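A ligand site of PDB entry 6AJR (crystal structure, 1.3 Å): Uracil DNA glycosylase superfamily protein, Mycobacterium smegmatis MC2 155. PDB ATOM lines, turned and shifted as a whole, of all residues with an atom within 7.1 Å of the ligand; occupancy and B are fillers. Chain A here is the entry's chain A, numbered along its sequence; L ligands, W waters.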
ATOM      1  N   VAL A  37       2.858 -18.399  30.277  1.00  0.00           N
ATOM      2  CA  VAL A  37       3.968 -18.925  29.493  1.00  0.00           C
ATOM      3  C   VAL A  37       5.233 -18.552  30.239  1.00  0.00           C
ATOM      4  O   VAL A  37       5.659 -17.392  30.233  1.00  0.00           O
ATOM      5  CB  VAL A  37       3.967 -18.387  28.059  1.00  0.00           C
ATOM      6  CG1 VAL A  37       5.163 -18.940  27.277  1.00  0.00           C
ATOM      7  CG2 VAL A  37       2.658 -18.744  27.350  1.00  0.00           C
ATOM      8  N   ILE A  50      15.019 -12.036  27.096  1.00  0.00           N
ATOM      9  CA  ILE A  50      13.719 -11.617  27.601  1.00  0.00           C
ATOM     10  C   ILE A  50      13.005 -10.828  26.523  1.00  0.00           C
ATOM     11  O   ILE A  50      13.505  -9.782  26.088  1.00  0.00           O
ATOM     12  CB  ILE A  50      13.844 -10.756  28.865  1.00  0.00           C
ATOM     13  CG1 ILE A  50      14.717 -11.440  29.936  1.00  0.00           C
ATOM     14  CG2 ILE A  50      12.460 -10.431  29.421  1.00  0.00           C
ATOM     15  CD1 ILE A  50      14.950 -10.606  31.181  1.00  0.00           C
ATOM     16  N   GLY A  51      11.837 -11.307  26.100  1.00  0.00           N
ATOM     17  CA  GLY A  51      10.959 -10.567  25.216  1.00  0.00           C
ATOM     18  C   GLY A  51       9.865  -9.831  25.977  1.00  0.00           C
ATOM     19  O   GLY A  51       9.953  -9.609  27.182  1.00  0.00           O
ATOM     20  N   GLU A  52       8.825  -9.444  25.236  1.00  0.00           N
ATOM     21  CA  GLU A  52       7.753  -8.654  25.815  1.00  0.00           C
ATOM     22  C   GLU A  52       6.728  -9.534  26.524  1.00  0.00           C
ATOM     23  O   GLU A  52       6.449  -9.353  27.725  1.00  0.00           O
ATOM     24  CB  GLU A  52       7.066  -7.807  24.746  1.00  0.00           C
ATOM     25  CG  GLU A  52       5.895  -7.013  25.304  1.00  0.00           C
ATOM     26  CD  GLU A  52       5.304  -6.077  24.288  1.00  0.00           C
ATOM     27  OE1 GLU A  52       5.724  -4.918  24.218  1.00  0.00           O
ATOM     28  OE2 GLU A  52       4.401  -6.506  23.546  1.00  0.00           O
ATOM     29  N   GLN A  53       6.115 -10.455  25.786  1.00  0.00           N
ATOM     30  CA  GLN A  53       5.006 -11.268  26.286  1.00  0.00           C
ATOM     31  C   GLN A  53       4.820 -12.417  25.315  1.00  0.00           C
ATOM     32  O   GLN A  53       5.253 -12.333  24.163  1.00  0.00           O
ATOM     33  CB  GLN A  53       3.708 -10.444  26.325  1.00  0.00           C
ATOM     34  CG  GLN A  53       3.236 -10.036  24.941  1.00  0.00           C
ATOM     35  CD  GLN A  53       1.954  -9.278  25.000  1.00  0.00           C
ATOM     36  OE1 GLN A  53       0.964  -9.797  25.484  1.00  0.00           O
ATOM     37  NE2 GLN A  53       1.955  -8.051  24.508  1.00  0.00           N
ATOM     38  N   PRO A  54       4.194 -13.512  25.753  1.00  0.00           N
ATOM     39  CA  PRO A  54       3.822 -14.550  24.787  1.00  0.00           C
ATOM     40  C   PRO A  54       2.808 -13.952  23.822  1.00  0.00           C
ATOM     41  O   PRO A  54       1.965 -13.150  24.216  1.00  0.00           O
ATOM     42  CB  PRO A  54       3.189 -15.630  25.663  1.00  0.00           C
ATOM     43  CG  PRO A  54       2.711 -14.924  26.882  1.00  0.00           C
ATOM     44  CD  PRO A  54       3.680 -13.803  27.109  1.00  0.00           C
ATOM     45  N   GLY A  55       2.930 -14.312  22.539  1.00  0.00           N
ATOM     46  CA  GLY A  55       1.932 -13.978  21.538  1.00  0.00           C
ATOM     47  C   GLY A  55       0.898 -15.077  21.350  1.00  0.00           C
ATOM     48  O   GLY A  55       0.771 -16.000  22.166  1.00  0.00           O
ATOM     49  N   ASP A  56       0.155 -14.976  20.250  1.00  0.00           N
ATOM     50  CA  ASP A  56      -0.931 -15.912  19.948  1.00  0.00           C
ATOM     51  C   ASP A  56      -0.436 -17.362  19.956  1.00  0.00           C
ATOM     52  O   ASP A  56      -1.016 -18.226  20.641  1.00  0.00           O
ATOM     53  CB  ASP A  56      -1.543 -15.534  18.594  1.00  0.00           C
ATOM     54  CG  ASP A  56      -2.847 -16.287  18.258  1.00  0.00           C
ATOM     55  OD1 ASP A  56      -3.293 -17.163  19.014  1.00  0.00           O
ATOM     56  OD2 ASP A  56      -3.427 -15.974  17.210  1.00  0.00           O
ATOM     57  N   GLU A  58       2.382 -18.618  21.214  1.00  0.00           N
ATOM     58  CA  GLU A  58       2.981 -18.987  22.497  1.00  0.00           C
ATOM     59  C   GLU A  58       1.912 -19.274  23.545  1.00  0.00           C
ATOM     60  O   GLU A  58       2.061 -20.196  24.363  1.00  0.00           O
ATOM     61  CB  GLU A  58       3.853 -17.835  22.998  1.00  0.00           C
ATOM     62  CG  GLU A  58       5.147 -17.625  22.200  1.00  0.00           C
ATOM     63  CD  GLU A  58       4.965 -16.975  20.836  1.00  0.00           C
ATOM     64  OE1 GLU A  58       3.924 -16.318  20.577  1.00  0.00           O
ATOM     65  OE2 GLU A  58       5.895 -17.122  20.020  1.00  0.00           O
ATOM     66  N   LEU A  63       5.009 -22.168  25.390  1.00  0.00           N
ATOM     67  CA  LEU A  63       6.450 -21.986  25.217  1.00  0.00           C
ATOM     68  C   LEU A  63       6.697 -20.633  24.579  1.00  0.00           C
ATOM     69  O   LEU A  63       5.897 -20.180  23.757  1.00  0.00           O
ATOM     70  CB  LEU A  63       7.012 -23.063  24.285  1.00  0.00           C
ATOM     71  CG  LEU A  63       6.883 -24.490  24.804  1.00  0.00           C
ATOM     72  CD1 LEU A  63       7.162 -25.481  23.678  1.00  0.00           C
ATOM     73  CD2 LEU A  63       7.825 -24.681  25.970  1.00  0.00           C
ATOM     74  N   PRO A  64       7.812 -19.983  24.911  1.00  0.00           N
ATOM     75  CA  PRO A  64       8.116 -18.675  24.322  1.00  0.00           C
ATOM     76  C   PRO A  64       8.721 -18.793  22.923  1.00  0.00           C
ATOM     77  O   PRO A  64       9.336 -19.801  22.564  1.00  0.00           O
ATOM     78  CB  PRO A  64       9.131 -18.089  25.297  1.00  0.00           C
ATOM     79  CG  PRO A  64       9.850 -19.298  25.852  1.00  0.00           C
ATOM     80  CD  PRO A  64       8.798 -20.371  25.936  1.00  0.00           C
ATOM     81  N   PHE A  65       8.526 -17.735  22.140  1.00  0.00           N
ATOM     82  CA  PHE A  65       9.191 -17.544  20.847  1.00  0.00           C
ATOM     83  C   PHE A  65       9.064 -18.773  19.943  1.00  0.00           C
ATOM     84  O   PHE A  65      10.057 -19.338  19.483  1.00  0.00           O
ATOM     85  CB  PHE A  65      10.647 -17.086  21.010  1.00  0.00           C
ATOM     86  CG  PHE A  65      10.769 -15.627  21.347  1.00  0.00           C
ATOM     87  CD1 PHE A  65      10.473 -14.658  20.396  1.00  0.00           C
ATOM     88  CD2 PHE A  65      11.191 -15.215  22.597  1.00  0.00           C
ATOM     89  CE1 PHE A  65      10.571 -13.307  20.696  1.00  0.00           C
ATOM     90  CE2 PHE A  65      11.295 -13.857  22.900  1.00  0.00           C
ATOM     91  CZ  PHE A  65      10.986 -12.915  21.940  1.00  0.00           C
ATOM     92  N   VAL A  66       7.813 -19.157  19.648  1.00  0.00           N
ATOM     93  CA  VAL A  66       7.513 -20.281  18.769  1.00  0.00           C
ATOM     94  C   VAL A  66       6.841 -19.867  17.480  1.00  0.00           C
ATOM     95  O   VAL A  66       6.618 -20.726  16.618  1.00  0.00           O
ATOM     96  CB  VAL A  66       6.720 -21.392  19.476  1.00  0.00           C
ATOM     97  CG1 VAL A  66       7.563 -22.026  20.575  1.00  0.00           C
ATOM     98  CG2 VAL A  66       5.395 -20.859  20.018  1.00  0.00           C
ATOM     99  N   GLY A  67       6.524 -18.595  17.308  1.00  0.00           N
ATOM    100  CA  GLY A  67       5.885 -18.112  16.105  1.00  0.00           C
ATOM    101  C   GLY A  67       6.879 -17.480  15.153  1.00  0.00           C
ATOM    102  O   GLY A  67       8.081 -17.734  15.211  1.00  0.00           O
ATOM    103  N   ALA A  69       8.190 -14.487  14.897  1.00  0.00           N
ATOM    104  CA  ALA A  69       9.292 -13.770  15.537  1.00  0.00           C
ATOM    105  C   ALA A  69      10.323 -14.737  16.092  1.00  0.00           C
ATOM    106  O   ALA A  69      11.527 -14.493  16.002  1.00  0.00           O
ATOM    107  CB  ALA A  69       8.739 -12.867  16.653  1.00  0.00           C
ATOM    108  N   GLY A  70       9.866 -15.866  16.646  1.00  0.00           N
ATOM    109  CA  GLY A  70      10.800 -16.860  17.138  1.00  0.00           C
ATOM    110  C   GLY A  70      11.613 -17.505  16.038  1.00  0.00           C
ATOM    111  O   GLY A  70      12.794 -17.812  16.225  1.00  0.00           O
ATOM    112  N   ARG A  84      20.249 -22.163  20.781  1.00  0.00           N
ATOM    113  CA  ARG A  84      19.066 -21.789  21.544  1.00  0.00           C
ATOM    114  C   ARG A  84      18.834 -22.711  22.741  1.00  0.00           C
ATOM    115  O   ARG A  84      18.338 -22.257  23.778  1.00  0.00           O
ATOM    116  CB  ARG A  84      17.835 -21.767  20.647  1.00  0.00           C
ATOM    117  CG  ARG A  84      16.600 -21.316  21.374  1.00  0.00           C
ATOM    118  CD  ARG A  84      15.416 -21.199  20.446  1.00  0.00           C
ATOM    119  NE  ARG A  84      14.195 -20.993  21.216  1.00  0.00           N
ATOM    120  CZ  ARG A  84      13.070 -20.465  20.734  1.00  0.00           C
ATOM    121  NH1 ARG A  84      12.992 -20.057  19.478  1.00  0.00           N
ATOM    122  NH2 ARG A  84      12.035 -20.341  21.541  1.00  0.00           N
ATOM    123  N   VAL A  89      15.103 -18.549  27.920  1.00  0.00           N
ATOM    124  CA  VAL A  89      14.316 -17.599  27.129  1.00  0.00           C
ATOM    125  C   VAL A  89      12.990 -17.351  27.829  1.00  0.00           C
ATOM    126  O   VAL A  89      12.262 -18.298  28.126  1.00  0.00           O
ATOM    127  CB  VAL A  89      14.093 -18.148  25.706  1.00  0.00           C
ATOM    128  CG1 VAL A  89      13.214 -17.190  24.907  1.00  0.00           C
ATOM    129  CG2 VAL A  89      15.434 -18.399  25.017  1.00  0.00           C
ATOM    130  N   THR A  90      12.666 -16.083  28.066  1.00  0.00           N
ATOM    131  CA  THR A  90      11.429 -15.755  28.783  1.00  0.00           C
ATOM    132  C   THR A  90      10.896 -14.427  28.269  1.00  0.00           C
ATOM    133  O   THR A  90      11.357 -13.907  27.244  1.00  0.00           O
ATOM    134  CB  THR A  90      11.656 -15.848  30.294  1.00  0.00           C
ATOM    135  OG1 THR A  90      10.398 -15.792  30.971  1.00  0.00           O
ATOM    136  CG2 THR A  90      12.585 -14.738  30.792  1.00  0.00           C
ATOM    137  N   ASN A  91       9.921 -13.868  28.991  1.00  0.00           N
ATOM    138  CA  ASN A  91       9.267 -12.618  28.630  1.00  0.00           C
ATOM    139  C   ASN A  91       9.019 -11.784  29.872  1.00  0.00           C
ATOM    140  O   ASN A  91       8.861 -12.314  30.979  1.00  0.00           O
ATOM    141  CB  ASN A  91       7.934 -12.869  27.935  1.00  0.00           C
ATOM    142  CG  ASN A  91       8.114 -13.439  26.550  1.00  0.00           C
ATOM    143  OD1 ASN A  91       8.625 -12.769  25.660  1.00  0.00           O
ATOM    144  ND2 ASN A  91       7.707 -14.684  26.369  1.00  0.00           N
ATOM    145  N   ALA A  92       8.906 -10.470  29.662  1.00  0.00           N
ATOM    146  CA  ALA A  92       8.672  -9.564  30.780  1.00  0.00           C
ATOM    147  C   ALA A  92       7.317  -9.795  31.434  1.00  0.00           C
ATOM    148  O   ALA A  92       7.187  -9.635  32.648  1.00  0.00           O
ATOM    149  CB  ALA A  92       8.793  -8.130  30.306  1.00  0.00           C
ATOM    150  N   VAL A  93       6.314 -10.154  30.651  1.00  0.00           N
ATOM    151  CA  VAL A  93       4.970 -10.443  31.148  1.00  0.00           C
ATOM    152  C   VAL A  93       4.622 -11.856  30.698  1.00  0.00           C
ATOM    153  O   VAL A  93       5.019 -12.280  29.607  1.00  0.00           O
ATOM    154  CB  VAL A  93       4.014  -9.381  30.562  1.00  0.00           C
ATOM    155  CG1 VAL A  93       2.581  -9.768  30.677  1.00  0.00           C
ATOM    156  CG2 VAL A  93       4.262  -8.067  31.294  1.00  0.00           C
ATOM    157  N   HIS A 109      -1.460  -8.945  19.635  1.00  0.00           N
ATOM    158  CA  HIS A 109      -0.961  -8.569  20.937  1.00  0.00           C
ATOM    159  C   HIS A 109      -1.149  -7.077  21.188  1.00  0.00           C
ATOM    160  O   HIS A 109      -1.116  -6.255  20.263  1.00  0.00           O
ATOM    161  CB  HIS A 109       0.513  -8.988  21.109  1.00  0.00           C
ATOM    162  CG  HIS A 109       1.427  -8.443  20.054  1.00  0.00           C
ATOM    163  ND1 HIS A 109       2.019  -7.210  20.158  1.00  0.00           N
ATOM    164  CD2 HIS A 109       1.892  -8.988  18.910  1.00  0.00           C
ATOM    165  CE1 HIS A 109       2.793  -6.992  19.106  1.00  0.00           C
ATOM    166  NE2 HIS A 109       2.730  -8.068  18.330  1.00  0.00           N
ATOM    167  N   LEU A 139      15.048  -8.014  24.553  1.00  0.00           N
ATOM    168  CA  LEU A 139      14.537  -7.950  23.188  1.00  0.00           C
ATOM    169  C   LEU A 139      13.357  -6.981  23.140  1.00  0.00           C
ATOM    170  O   LEU A 139      12.243  -7.342  23.519  1.00  0.00           O
ATOM    171  CB  LEU A 139      14.111  -9.336  22.716  1.00  0.00           C
ATOM    172  CG  LEU A 139      15.190 -10.417  22.662  1.00  0.00           C
ATOM    173  CD1 LEU A 139      14.545 -11.797  22.550  1.00  0.00           C
ATOM    174  CD2 LEU A 139      16.184 -10.170  21.527  1.00  0.00           C
ATOM    175  N   HIS A 178      13.490  -5.949  19.003  1.00  0.00           N
ATOM    176  CA  HIS A 178      12.667  -7.142  19.112  1.00  0.00           C
ATOM    177  C   HIS A 178      12.573  -7.826  17.750  1.00  0.00           C
ATOM    178  O   HIS A 178      12.386  -7.159  16.729  1.00  0.00           O
ATOM    179  CB  HIS A 178      11.276  -6.765  19.580  1.00  0.00           C
ATOM    180  CG  HIS A 178      10.454  -7.937  20.002  1.00  0.00           C
ATOM    181  ND1 HIS A 178       9.907  -8.822  19.097  1.00  0.00           N
ATOM    182  CD2 HIS A 178      10.094  -8.378  21.223  1.00  0.00           C
ATOM    183  CE1 HIS A 178       9.223  -9.747  19.751  1.00  0.00           C
ATOM    184  NE2 HIS A 178       9.338  -9.509  21.047  1.00  0.00           N
ATOM    185  N   PRO A 179      12.684  -9.165  17.698  1.00  0.00           N
ATOM    186  CA  PRO A 179      12.624  -9.828  16.385  1.00  0.00           C
ATOM    187  C   PRO A 179      11.355  -9.561  15.603  1.00  0.00           C
ATOM    188  O   PRO A 179      11.396  -9.583  14.371  1.00  0.00           O
ATOM    189  CB  PRO A 179      12.775 -11.326  16.723  1.00  0.00           C
ATOM    190  CG  PRO A 179      12.480 -11.432  18.174  1.00  0.00           C
ATOM    191  CD  PRO A 179      12.971 -10.126  18.778  1.00  0.00           C
ATOM    192  N   SER A 180      10.227  -9.311  16.272  1.00  0.00           N
ATOM    193  CA  SER A 180       8.999  -9.029  15.537  1.00  0.00           C
ATOM    194  C   SER A 180       9.131  -7.770  14.698  1.00  0.00           C
ATOM    195  O   SER A 180       8.515  -7.672  13.619  1.00  0.00           O
ATOM    196  CB  SER A 180       7.800  -8.941  16.500  1.00  0.00           C
ATOM    197  OG  SER A 180       7.960  -7.883  17.430  1.00  0.00           O
HETATM  198  N1  LIG L   1       6.968 -11.991  21.100  1.00  0.00           N
HETATM  199  C1  LIG L   1       7.582 -11.916  22.438  1.00  0.00           C
HETATM  200  O1  LIG L   1       7.919 -10.908  22.961  1.00  0.00           O
HETATM  201  N2  LIG L   1       7.831 -13.122  23.203  1.00  0.00           N
HETATM  202  C2  LIG L   1       7.444 -14.410  22.711  1.00  0.00           C
HETATM  203  O2  LIG L   1       7.673 -15.338  23.401  1.00  0.00           O
HETATM  204  C3  LIG L   1       6.837 -14.473  21.356  1.00  0.00           C
HETATM  205  C4  LIG L   1       6.596 -13.286  20.585  1.00  0.00           C
HETATM  206  O   HOH W   1       3.726 -11.062  21.713  1.00  0.00           O
HETATM  207  O   HOH W   2       3.644 -12.174  19.076  1.00  0.00           O
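OD1 of Asn 91 lies within hydrogen-bond range of N of Gln 53 (3.4 Å). The backbone carbonyl oxygen of Glu 52 lies within hydrogen-bond range of the backbone NH of Val 93, 3.0 Å away. NH2 of Arg 84 is in hydrogen-bond range of O of Pro 64, 2.9 Å away. The backbone NH (N) of Ala 92 is in hydrogen-bond range of the backbone carbonyl oxygen (O) of Glu 52 (3.3 Å). The side-chain carboxylate (OE2) of Glu 52 sits at hydrogen-bond distance from the side-chain amide nitrogen (NE2) of Gln 53, 3.0 Å away. OE2 of Glu 58 sits at hydrogen-bond distance from N of Gly 67. OE1 of Glu 58 sits at hydrogen-bond distance from N of Gly 55. The side-chain amide oxygen (OD1) of Asn 91 sits at hydrogen-bond distance from the backbone NH (N) of Glu 52 (3.4 Å).
N of Gln 53 lies within hydrogen-bond range of O1 of the ligand. N of Glu 52 lies within hydrogen-bond range of O1 of the ligand, 2.9 Å away. NE2 of His 178 is in hydrogen-bond range of O1 of the ligand, 2.8 Å away. The backbone carbonyl oxygen of Gln 53 is in hydrogen-bond range of a nitrogen (N2) of the ligand, 2.9 Å away. The backbone NH of Phe 65 is in hydrogen-bond range of an oxygen (O2) of the ligand, 2.8 Å away. OD1 of Asn 91 lies within hydrogen-bond range of N2 of the ligand (2.6 Å).
Residues that only touch the ligand: Gly 51 (3.7 Å), Glu 58 (3.1 Å) and Pro 64 (3.5 Å). Hydrophobic or aromatic side chains within 4 Å of the ligand: Pro 64, Phe 65 and His 178. Eight residues have an atom within 4 Å of the ligand: Gly 51, Glu 52, Gln 53, Glu 58, Pro 64, Phe 65, Asn 91 and His 178.
Water W1 lies within hydrogen-bond range of the backbone carbonyl oxygen of Gln 53 (3.2 Å), a nitrogen (N1) of the ligand (3.4 Å) and the backbone NH of Gly 55 (3.4 Å).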
